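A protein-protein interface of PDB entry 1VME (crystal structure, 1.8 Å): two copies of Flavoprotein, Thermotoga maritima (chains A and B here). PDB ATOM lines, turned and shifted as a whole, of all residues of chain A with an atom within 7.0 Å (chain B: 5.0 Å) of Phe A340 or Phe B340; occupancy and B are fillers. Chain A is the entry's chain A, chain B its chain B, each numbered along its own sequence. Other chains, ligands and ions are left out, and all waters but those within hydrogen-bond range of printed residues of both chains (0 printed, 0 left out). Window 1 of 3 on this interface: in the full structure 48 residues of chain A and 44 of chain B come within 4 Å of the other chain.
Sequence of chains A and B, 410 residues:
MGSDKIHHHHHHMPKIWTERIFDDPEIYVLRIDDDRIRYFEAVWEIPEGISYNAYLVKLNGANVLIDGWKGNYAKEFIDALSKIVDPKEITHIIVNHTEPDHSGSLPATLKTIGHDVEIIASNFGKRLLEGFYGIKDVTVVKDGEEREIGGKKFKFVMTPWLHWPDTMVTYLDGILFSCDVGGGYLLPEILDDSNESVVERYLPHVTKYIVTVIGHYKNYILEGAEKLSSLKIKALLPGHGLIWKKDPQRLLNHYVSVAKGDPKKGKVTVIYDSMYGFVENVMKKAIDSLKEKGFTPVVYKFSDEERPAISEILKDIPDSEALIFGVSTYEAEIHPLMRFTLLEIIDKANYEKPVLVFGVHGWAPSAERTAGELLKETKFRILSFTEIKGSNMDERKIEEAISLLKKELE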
ATOM      1  N   VAL A  43     -21.334 -21.744  25.052  1.00  0.00           N
ATOM      2  CA  VAL A  43     -20.671 -20.767  24.216  1.00  0.00           C
ATOM      3  C   VAL A  43     -21.584 -19.728  23.555  1.00  0.00           C
ATOM      4  O   VAL A  43     -21.257 -18.547  23.558  1.00  0.00           O
ATOM      5  CB  VAL A  43     -19.726 -21.431  23.168  1.00  0.00           C
ATOM      6  CG1 VAL A  43     -20.382 -22.429  22.416  1.00  0.00           C
ATOM      7  CG2 VAL A  43     -19.124 -20.362  22.202  1.00  0.00           C
ATOM      8  N   TRP A  44     -22.732 -20.114  23.001  1.00  0.00           N
ATOM      9  CA  TRP A  44     -23.504 -19.177  22.146  1.00  0.00           C
ATOM     10  C   TRP A  44     -24.495 -18.355  22.948  1.00  0.00           C
ATOM     11  O   TRP A  44     -25.394 -18.896  23.554  1.00  0.00           O
ATOM     12  CB  TRP A  44     -24.267 -19.927  21.068  1.00  0.00           C
ATOM     13  CG  TRP A  44     -23.394 -20.913  20.395  1.00  0.00           C
ATOM     14  CD1 TRP A  44     -23.554 -22.253  20.415  1.00  0.00           C
ATOM     15  CD2 TRP A  44     -22.183 -20.658  19.655  1.00  0.00           C
ATOM     16  NE1 TRP A  44     -22.531 -22.856  19.736  1.00  0.00           N
ATOM     17  CE2 TRP A  44     -21.678 -21.905  19.260  1.00  0.00           C
ATOM     18  CE3 TRP A  44     -21.477 -19.493  19.295  1.00  0.00           C
ATOM     19  CZ2 TRP A  44     -20.484 -22.038  18.524  1.00  0.00           C
ATOM     20  CZ3 TRP A  44     -20.313 -19.606  18.581  1.00  0.00           C
ATOM     21  CH2 TRP A  44     -19.810 -20.882  18.209  1.00  0.00           C
ATOM     22  N   GLU A  45     -24.340 -17.051  22.909  1.00  0.00           N
ATOM     23  CA  GLU A  45     -25.171 -16.147  23.714  1.00  0.00           C
ATOM     24  C   GLU A  45     -26.622 -16.200  23.210  1.00  0.00           C
ATOM     25  O   GLU A  45     -26.894 -15.866  22.047  1.00  0.00           O
ATOM     26  CB  GLU A  45     -24.628 -14.717  23.593  1.00  0.00           C
ATOM     27  CG  GLU A  45     -23.142 -14.577  23.884  1.00  0.00           C
ATOM     28  CD  GLU A  45     -22.157 -14.737  22.643  1.00  0.00           C
ATOM     29  OE1 GLU A  45     -22.380 -15.516  21.680  1.00  0.00           O
ATOM     30  OE2 GLU A  45     -21.068 -14.106  22.742  1.00  0.00           O
ATOM     31  N   PHE A 302     -15.842  -4.256  18.135  1.00  0.00           N
ATOM     32  CA  PHE A 302     -15.179  -4.551  19.387  1.00  0.00           C
ATOM     33  C   PHE A 302     -14.390  -3.282  19.783  1.00  0.00           C
ATOM     34  O   PHE A 302     -13.438  -2.906  19.088  1.00  0.00           O
ATOM     35  CB  PHE A 302     -14.207  -5.685  19.266  1.00  0.00           C
ATOM     36  CG  PHE A 302     -14.844  -7.003  18.970  1.00  0.00           C
ATOM     37  CD1 PHE A 302     -15.279  -7.820  19.995  1.00  0.00           C
ATOM     38  CD2 PHE A 302     -15.015  -7.407  17.676  1.00  0.00           C
ATOM     39  CE1 PHE A 302     -15.879  -9.057  19.709  1.00  0.00           C
ATOM     40  CE2 PHE A 302     -15.624  -8.642  17.384  1.00  0.00           C
ATOM     41  CZ  PHE A 302     -16.029  -9.459  18.405  1.00  0.00           C
ATOM     42  N   ARG A 307     -18.730  -4.867  23.247  1.00  0.00           N
ATOM     43  CA  ARG A 307     -18.291  -6.184  22.770  1.00  0.00           C
ATOM     44  C   ARG A 307     -19.525  -6.903  22.223  1.00  0.00           C
ATOM     45  O   ARG A 307     -20.438  -7.183  22.979  1.00  0.00           O
ATOM     46  CB  ARG A 307     -17.790  -6.950  23.965  1.00  0.00           C
ATOM     47  CG  ARG A 307     -17.429  -8.360  23.560  1.00  0.00           C
ATOM     48  CD  ARG A 307     -16.496  -8.917  24.469  1.00  0.00           C
ATOM     49  NE  ARG A 307     -15.354  -8.040  24.523  1.00  0.00           N
ATOM     50  CZ  ARG A 307     -14.342  -8.251  25.335  1.00  0.00           C
ATOM     51  NH1 ARG A 307     -14.337  -9.332  26.124  1.00  0.00           N
ATOM     52  NH2 ARG A 307     -13.331  -7.407  25.315  1.00  0.00           N
ATOM     53  N   ILE A 310     -20.766 -13.230  19.780  1.00  0.00           N
ATOM     54  CA  ILE A 310     -20.368 -13.936  18.601  1.00  0.00           C
ATOM     55  C   ILE A 310     -21.532 -14.617  17.912  1.00  0.00           C
ATOM     56  O   ILE A 310     -21.573 -14.708  16.707  1.00  0.00           O
ATOM     57  CB  ILE A 310     -19.208 -14.936  18.888  1.00  0.00           C
ATOM     58  CG1 ILE A 310     -18.715 -15.644  17.650  1.00  0.00           C
ATOM     59  CG2 ILE A 310     -19.637 -15.997  19.909  1.00  0.00           C
ATOM     60  CD1 ILE A 310     -18.120 -14.797  16.577  1.00  0.00           C
ATOM     61  N   ILE A 334      -2.975 -10.691  15.336  1.00  0.00           N
ATOM     62  CA  ILE A 334      -4.026  -9.680  15.377  1.00  0.00           C
ATOM     63  C   ILE A 334      -4.750  -9.673  16.715  1.00  0.00           C
ATOM     64  O   ILE A 334      -4.466 -10.475  17.601  1.00  0.00           O
ATOM     65  CB  ILE A 334      -5.044  -9.833  14.224  1.00  0.00           C
ATOM     66  CG1 ILE A 334      -5.751 -11.197  14.266  1.00  0.00           C
ATOM     67  CG2 ILE A 334      -4.349  -9.606  12.897  1.00  0.00           C
ATOM     68  CD1 ILE A 334      -6.956 -11.310  13.310  1.00  0.00           C
ATOM     69  N   HIS A 335      -5.675  -8.740  16.860  1.00  0.00           N
ATOM     70  CA  HIS A 335      -6.444  -8.592  18.088  1.00  0.00           C
ATOM     71  C   HIS A 335      -7.159  -9.906  18.386  1.00  0.00           C
ATOM     72  O   HIS A 335      -7.752 -10.486  17.466  1.00  0.00           O
ATOM     73  CB  HIS A 335      -7.446  -7.476  17.878  1.00  0.00           C
ATOM     74  CG  HIS A 335      -8.149  -7.035  19.128  1.00  0.00           C
ATOM     75  ND1 HIS A 335      -9.176  -7.757  19.699  1.00  0.00           N
ATOM     76  CD2 HIS A 335      -7.960  -5.951  19.916  1.00  0.00           C
ATOM     77  CE1 HIS A 335      -9.598  -7.122  20.778  1.00  0.00           C
ATOM     78  NE2 HIS A 335      -8.858  -6.035  20.943  1.00  0.00           N
ATOM     79  N   PRO A 336      -7.030 -10.423  19.630  1.00  0.00           N
ATOM     80  CA  PRO A 336      -7.562 -11.677  20.248  1.00  0.00           C
ATOM     81  C   PRO A 336      -9.068 -11.985  20.071  1.00  0.00           C
ATOM     82  O   PRO A 336      -9.486 -13.095  19.722  1.00  0.00           O
ATOM     83  CB  PRO A 336      -7.238 -11.472  21.723  1.00  0.00           C
ATOM     84  CG  PRO A 336      -6.016 -10.679  21.699  1.00  0.00           C
ATOM     85  CD  PRO A 336      -6.153  -9.709  20.579  1.00  0.00           C
ATOM     86  N   LEU A 337      -9.852 -10.912  20.167  1.00  0.00           N
ATOM     87  CA  LEU A 337     -11.281 -11.068  19.858  1.00  0.00           C
ATOM     88  C   LEU A 337     -11.536 -11.167  18.371  1.00  0.00           C
ATOM     89  O   LEU A 337     -12.472 -11.880  17.954  1.00  0.00           O
ATOM     90  CB  LEU A 337     -12.137  -9.977  20.477  1.00  0.00           C
ATOM     91  CG  LEU A 337     -11.993  -9.893  22.006  1.00  0.00           C
ATOM     92  CD1 LEU A 337     -12.770  -8.705  22.470  1.00  0.00           C
ATOM     93  CD2 LEU A 337     -12.494 -11.132  22.655  1.00  0.00           C
ATOM     94  N   MET A 338     -10.715 -10.538  17.543  1.00  0.00           N
ATOM     95  CA  MET A 338     -10.824 -10.679  16.112  1.00  0.00           C
ATOM     96  C   MET A 338     -10.382 -12.101  15.681  1.00  0.00           C
ATOM     97  O   MET A 338     -10.936 -12.693  14.756  1.00  0.00           O
ATOM     98  CB  MET A 338      -9.948  -9.619  15.454  1.00  0.00           C
ATOM     99  CG  MET A 338      -9.917  -9.623  13.948  1.00  0.00           C
ATOM    100  SD  MET A 338     -11.712  -9.641  13.088  1.00  0.00           S
ATOM    101  CE  MET A 338     -12.696  -8.330  14.179  1.00  0.00           C
ATOM    102  N   ARG A 339      -9.344 -12.623  16.328  1.00  0.00           N
ATOM    103  CA  ARG A 339      -8.912 -13.999  16.104  1.00  0.00           C
ATOM    104  C   ARG A 339     -10.083 -14.947  16.393  1.00  0.00           C
ATOM    105  O   ARG A 339     -10.417 -15.811  15.580  1.00  0.00           O
ATOM    106  CB  ARG A 339      -7.715 -14.362  16.948  1.00  0.00           C
ATOM    107  CG  ARG A 339      -7.206 -15.729  16.612  1.00  0.00           C
ATOM    108  CD  ARG A 339      -6.258 -16.233  17.665  1.00  0.00           C
ATOM    109  NE  ARG A 339      -6.904 -16.459  18.957  1.00  0.00           N
ATOM    110  CZ  ARG A 339      -6.538 -15.912  20.105  1.00  0.00           C
ATOM    111  NH1 ARG A 339      -5.513 -15.048  20.167  1.00  0.00           N
ATOM    112  NH2 ARG A 339      -7.179 -16.235  21.208  1.00  0.00           N
ATOM    113  N   PHE A 340     -10.706 -14.802  17.556  1.00  0.00           N
ATOM    114  CA  PHE A 340     -11.772 -15.709  17.932  1.00  0.00           C
ATOM    115  C   PHE A 340     -12.912 -15.644  16.916  1.00  0.00           C
ATOM    116  O   PHE A 340     -13.449 -16.666  16.479  1.00  0.00           O
ATOM    117  CB  PHE A 340     -12.305 -15.302  19.296  1.00  0.00           C
ATOM    118  CG  PHE A 340     -13.410 -16.173  19.784  1.00  0.00           C
ATOM    119  CD1 PHE A 340     -13.132 -17.318  20.491  1.00  0.00           C
ATOM    120  CD2 PHE A 340     -14.742 -15.817  19.598  1.00  0.00           C
ATOM    121  CE1 PHE A 340     -14.135 -18.160  20.960  1.00  0.00           C
ATOM    122  CE2 PHE A 340     -15.742 -16.618  20.086  1.00  0.00           C
ATOM    123  CZ  PHE A 340     -15.461 -17.806  20.738  1.00  0.00           C
ATOM    124  N   THR A 341     -13.273 -14.427  16.567  1.00  0.00           N
ATOM    125  CA  THR A 341     -14.351 -14.180  15.591  1.00  0.00           C
ATOM    126  C   THR A 341     -14.050 -14.821  14.245  1.00  0.00           C
ATOM    127  O   THR A 341     -14.874 -15.549  13.665  1.00  0.00           O
ATOM    128  CB  THR A 341     -14.654 -12.666  15.470  1.00  0.00           C
ATOM    129  OG1 THR A 341     -15.074 -12.155  16.712  1.00  0.00           O
ATOM    130  CG2 THR A 341     -15.693 -12.437  14.446  1.00  0.00           C
ATOM    131  N   LEU A 342     -12.843 -14.604  13.728  1.00  0.00           N
ATOM    132  CA  LEU A 342     -12.482 -15.194  12.448  1.00  0.00           C
ATOM    133  C   LEU A 342     -12.476 -16.712  12.497  1.00  0.00           C
ATOM    134  O   LEU A 342     -12.956 -17.368  11.569  1.00  0.00           O
ATOM    135  CB  LEU A 342     -11.143 -14.697  11.994  1.00  0.00           C
ATOM    136  CG  LEU A 342     -11.147 -13.248  11.509  1.00  0.00           C
ATOM    137  CD1 LEU A 342      -9.720 -12.813  11.197  1.00  0.00           C
ATOM    138  CD2 LEU A 342     -12.033 -13.075  10.289  1.00  0.00           C
ATOM    139  N   LEU A 343     -11.910 -17.285  13.554  1.00  0.00           N
ATOM    140  CA  LEU A 343     -11.896 -18.724  13.663  1.00  0.00           C
ATOM    141  C   LEU A 343     -13.320 -19.313  13.713  1.00  0.00           C
ATOM    142  O   LEU A 343     -13.557 -20.379  13.164  1.00  0.00           O
ATOM    143  CB  LEU A 343     -11.104 -19.179  14.891  1.00  0.00           C
ATOM    144  CG  LEU A 343      -9.626 -18.938  14.859  1.00  0.00           C
ATOM    145  CD1 LEU A 343      -8.964 -19.406  16.127  1.00  0.00           C
ATOM    146  CD2 LEU A 343      -9.008 -19.667  13.675  1.00  0.00           C
ATOM    147  N   GLU A 344     -14.237 -18.640  14.396  1.00  0.00           N
ATOM    148  CA  GLU A 344     -15.642 -19.133  14.470  1.00  0.00           C
ATOM    149  C   GLU A 344     -16.403 -18.961  13.146  1.00  0.00           C
ATOM    150  O   GLU A 344     -17.151 -19.839  12.709  1.00  0.00           O
ATOM    151  CB  GLU A 344     -16.378 -18.485  15.625  1.00  0.00           C
ATOM    152  CG  GLU A 344     -15.806 -18.873  16.971  1.00  0.00           C
ATOM    153  CD  GLU A 344     -15.670 -20.372  17.125  1.00  0.00           C
ATOM    154  OE1 GLU A 344     -16.582 -21.116  16.698  1.00  0.00           O
ATOM    155  OE2 GLU A 344     -14.600 -20.835  17.604  1.00  0.00           O
ATOM    156  N   ILE A 345     -16.118 -17.857  12.462  1.00  0.00           N
ATOM    157  CA  ILE A 345     -16.653 -17.664  11.074  1.00  0.00           C
ATOM    158  C   ILE A 345     -16.127 -18.741  10.165  1.00  0.00           C
ATOM    159  O   ILE A 345     -16.876 -19.344   9.365  1.00  0.00           O
ATOM    160  CB  ILE A 345     -16.372 -16.235  10.563  1.00  0.00           C
ATOM    161  CG1 ILE A 345     -17.178 -15.191  11.306  1.00  0.00           C
ATOM    162  CG2 ILE A 345     -16.665 -16.190   9.022  1.00  0.00           C
ATOM    163  CD1 ILE A 345     -16.760 -13.757  11.017  1.00  0.00           C
ATOM    164  N   ILE A 346     -14.852 -19.033  10.246  1.00  0.00           N
ATOM    165  CA  ILE A 346     -14.298 -20.103   9.428  1.00  0.00           C
ATOM    166  C   ILE A 346     -14.938 -21.450   9.747  1.00  0.00           C
ATOM    167  O   ILE A 346     -15.206 -22.257   8.845  1.00  0.00           O
ATOM    168  CB  ILE A 346     -12.779 -20.142   9.525  1.00  0.00           C
ATOM    169  CG1 ILE A 346     -12.229 -18.853   8.879  1.00  0.00           C
ATOM    170  CG2 ILE A 346     -12.227 -21.385   8.908  1.00  0.00           C
ATOM    171  CD1 ILE A 346     -10.769 -18.638   9.246  1.00  0.00           C
ATOM    172  N   ILE B 310     -11.464 -13.518  30.863  1.00  0.00           N
ATOM    173  CA  ILE B 310     -10.135 -14.013  30.618  1.00  0.00           C
ATOM    174  C   ILE B 310      -9.082 -13.224  31.381  1.00  0.00           C
ATOM    175  O   ILE B 310      -8.121 -13.792  31.817  1.00  0.00           O
ATOM    176  CB  ILE B 310      -9.784 -14.073  29.111  1.00  0.00           C
ATOM    177  CG1 ILE B 310      -8.431 -14.698  28.858  1.00  0.00           C
ATOM    178  CG2 ILE B 310      -9.801 -12.676  28.481  1.00  0.00           C
ATOM    179  CD1 ILE B 310      -8.348 -16.152  29.230  1.00  0.00           C
ATOM    180  N   PRO B 336     -14.433 -24.204  22.231  1.00  0.00           N
ATOM    181  CA  PRO B 336     -14.020 -22.882  21.682  1.00  0.00           C
ATOM    182  C   PRO B 336     -13.554 -21.803  22.720  1.00  0.00           C
ATOM    183  O   PRO B 336     -12.569 -21.057  22.546  1.00  0.00           O
ATOM    184  CB  PRO B 336     -15.284 -22.399  20.984  1.00  0.00           C
ATOM    185  CG  PRO B 336     -16.070 -23.584  20.683  1.00  0.00           C
ATOM    186  CD  PRO B 336     -15.775 -24.600  21.759  1.00  0.00           C
ATOM    187  N   LEU B 337     -14.224 -21.815  23.856  1.00  0.00           N
ATOM    188  CA  LEU B 337     -13.762 -20.958  24.975  1.00  0.00           C
ATOM    189  C   LEU B 337     -12.518 -21.505  25.637  1.00  0.00           C
ATOM    190  O   LEU B 337     -11.704 -20.708  26.146  1.00  0.00           O
ATOM    191  CB  LEU B 337     -14.876 -20.678  26.011  1.00  0.00           C
ATOM    192  CG  LEU B 337     -16.076 -19.924  25.413  1.00  0.00           C
ATOM    193  CD1 LEU B 337     -17.072 -19.650  26.506  1.00  0.00           C
ATOM    194  CD2 LEU B 337     -15.695 -18.652  24.735  1.00  0.00           C
ATOM    195  N   MET B 338     -12.335 -22.816  25.637  1.00  0.00           N
ATOM    196  CA  MET B 338     -11.106 -23.384  26.176  1.00  0.00           C
ATOM    197  C   MET B 338      -9.954 -23.131  25.199  1.00  0.00           C
ATOM    198  O   MET B 338      -8.830 -22.893  25.615  1.00  0.00           O
ATOM    199  CB  MET B 338     -11.251 -24.851  26.559  1.00  0.00           C
ATOM    200  CG  MET B 338     -12.192 -25.074  27.789  1.00  0.00           C
ATOM    201  SD  MET B 338     -11.459 -24.279  29.441  1.00  0.00           S
ATOM    202  CE  MET B 338     -10.191 -25.757  29.933  1.00  0.00           C
ATOM    203  N   ARG B 339     -10.240 -23.207  23.907  1.00  0.00           N
ATOM    204  CA  ARG B 339      -9.243 -22.847  22.903  1.00  0.00           C
ATOM    205  C   ARG B 339      -8.751 -21.415  23.151  1.00  0.00           C
ATOM    206  O   ARG B 339      -7.528 -21.171  23.209  1.00  0.00           O
ATOM    207  CB  ARG B 339      -9.825 -22.934  21.513  1.00  0.00           C
ATOM    208  CG  ARG B 339      -8.757 -22.689  20.423  1.00  0.00           C
ATOM    209  CD  ARG B 339      -9.375 -22.474  19.078  1.00  0.00           C
ATOM    210  NE  ARG B 339     -10.164 -21.261  19.006  1.00  0.00           N
ATOM    211  CZ  ARG B 339     -11.416 -21.157  18.569  1.00  0.00           C
ATOM    212  NH1 ARG B 339     -12.094 -22.195  18.111  1.00  0.00           N
ATOM    213  NH2 ARG B 339     -12.003 -19.990  18.588  1.00  0.00           N
ATOM    214  N   PHE B 340      -9.687 -20.480  23.239  1.00  0.00           N
ATOM    215  CA  PHE B 340      -9.366 -19.074  23.422  1.00  0.00           C
ATOM    216  C   PHE B 340      -8.537 -18.865  24.685  1.00  0.00           C
ATOM    217  O   PHE B 340      -7.516 -18.151  24.692  1.00  0.00           O
ATOM    218  CB  PHE B 340     -10.658 -18.261  23.523  1.00  0.00           C
ATOM    219  CG  PHE B 340     -10.432 -16.812  23.766  1.00  0.00           C
ATOM    220  CD1 PHE B 340     -10.195 -15.973  22.733  1.00  0.00           C
ATOM    221  CD2 PHE B 340     -10.421 -16.282  25.046  1.00  0.00           C
ATOM    222  CE1 PHE B 340      -9.971 -14.624  22.915  1.00  0.00           C
ATOM    223  CE2 PHE B 340     -10.208 -14.909  25.245  1.00  0.00           C
ATOM    224  CZ  PHE B 340      -9.982 -14.081  24.181  1.00  0.00           C
ATOM    225  N   THR B 341      -8.994 -19.491  25.756  1.00  0.00           N
ATOM    226  CA  THR B 341      -8.308 -19.416  27.050  1.00  0.00           C
ATOM    227  C   THR B 341      -6.894 -19.964  26.964  1.00  0.00           C
ATOM    228  O   THR B 341      -5.954 -19.310  27.430  1.00  0.00           O
ATOM    229  CB  THR B 341      -9.106 -20.116  28.145  1.00  0.00           C
ATOM    230  OG1 THR B 341     -10.348 -19.447  28.254  1.00  0.00           O
ATOM    231  CG2 THR B 341      -8.421 -20.035  29.469  1.00  0.00           C
ATOM    232  N   LEU B 342      -6.745 -21.169  26.425  1.00  0.00           N
ATOM    233  CA  LEU B 342      -5.418 -21.749  26.278  1.00  0.00           C
ATOM    234  C   LEU B 342      -4.514 -20.863  25.431  1.00  0.00           C
ATOM    235  O   LEU B 342      -3.329 -20.651  25.782  1.00  0.00           O
ATOM    236  CB  LEU B 342      -5.477 -23.149  25.683  1.00  0.00           C
ATOM    237  CG  LEU B 342      -5.948 -24.214  26.672  1.00  0.00           C
ATOM    238  CD1 LEU B 342      -6.189 -25.503  25.886  1.00  0.00           C
ATOM    239  CD2 LEU B 342      -4.947 -24.446  27.744  1.00  0.00           C
ATOM    240  N   LEU B 343      -5.021 -20.340  24.329  1.00  0.00           N
ATOM    241  CA  LEU B 343      -4.183 -19.501  23.462  1.00  0.00           C
ATOM    242  C   LEU B 343      -3.715 -18.244  24.187  1.00  0.00           C
ATOM    243  O   LEU B 343      -2.569 -17.793  23.990  1.00  0.00           O
ATOM    244  CB  LEU B 343      -4.885 -19.142  22.205  1.00  0.00           C
ATOM    245  CG  LEU B 343      -5.096 -20.293  21.207  1.00  0.00           C
ATOM    246  CD1 LEU B 343      -5.919 -19.886  20.063  1.00  0.00           C
ATOM    247  CD2 LEU B 343      -3.735 -20.788  20.736  1.00  0.00           C
ATOM    248  N   GLU B 344      -4.589 -17.653  24.984  1.00  0.00           N
ATOM    249  CA  GLU B 344      -4.200 -16.457  25.769  1.00  0.00           C
ATOM    250  C   GLU B 344      -3.201 -16.767  26.899  1.00  0.00           C
ATOM    251  O   GLU B 344      -2.259 -16.018  27.144  1.00  0.00           O
ATOM    252  CB  GLU B 344      -5.418 -15.749  26.304  1.00  0.00           C
ATOM    253  CG  GLU B 344      -6.263 -15.088  25.175  1.00  0.00           C
ATOM    254  CD  GLU B 344      -5.443 -14.240  24.243  1.00  0.00           C
ATOM    255  OE1 GLU B 344      -4.588 -13.454  24.711  1.00  0.00           O
ATOM    256  OE2 GLU B 344      -5.580 -14.416  23.007  1.00  0.00           O
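Printed residues of chain B within 4 Å of Arg A339: Phe B340 (3.4 Å), Leu B343 (3.7 Å) and Glu B344 (2.9 Å). Printed residues of chain B within 4 Å of Phe A340: Pro B336, Arg B339 and Phe B340. Printed residues of chain B within 4 Å of Leu A343: Arg B339. Printed residues of chain B within 4 Å of Glu A344: Pro B336 (3.8 Å) and Arg B339 (2.9 Å). Printed residues of chain A within 4 Å of Pro B336: Phe A340 (3.7 Å) and Glu A344 (3.8 Å). Of the printed residues of chain A, Phe B340 touches Pro A336, Arg A339 and Phe A340. The nearest printed residue of chain A that does not touch Phe B340 is Leu A337 (4.2 Å). The nearest printed residue of chain B that does not touch Leu A343 is Leu B343 (5.0 Å).
The guanidinium group of Arg A339 lies within salt-bridge range of the side-chain carboxylate of Glu B344 (2.9 Å). NH1 of Arg B339 lies within salt-bridge range of OE2 of Glu A344, at 2.9 Å.
Pro A336 touches Glu B344, and with the chains exchanged Glu A344 touches Pro B336. Arg A339 touches Phe B340, and with the chains exchanged Phe A340 touches Arg B339. Arg A339 touches Glu B344, and with the chains exchanged Glu A344 touches Arg B339. Phe A340 touches its own counterpart, Phe B340. Of the 11 pairs that touch across the chains among the printed residues, 11 have their exchanged pair printed and touching as well.
Among the printed residues, merely in contact across the chains: Arg A339 with Phe B340, Phe A340 with Arg B339, Pro A336 with Phe B340, Pro A336 with Glu B344, Leu A343 with Arg B339, Phe A340 with Pro B336, Arg A339 with Leu B343, Glu A344 with Pro B336 and Phe A340 with Phe B340.
Printed residues of chain B that touch a printed residue of chain A: Pro B336, Arg B339, Phe B340, Leu B343 and Glu B344. Hydrophobic or aromatic side chains of chain B that line the printed part of chain A: Pro B336, Phe B340 and Leu B343. Among the printed residues, Asp or Glu carboxylates within 4 Å of a Lys or Arg side-chain nitrogen of the other chain: Arg A339 with Glu B344 (2.9 Å) and Glu A344 with Arg B339 (2.9 Å).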
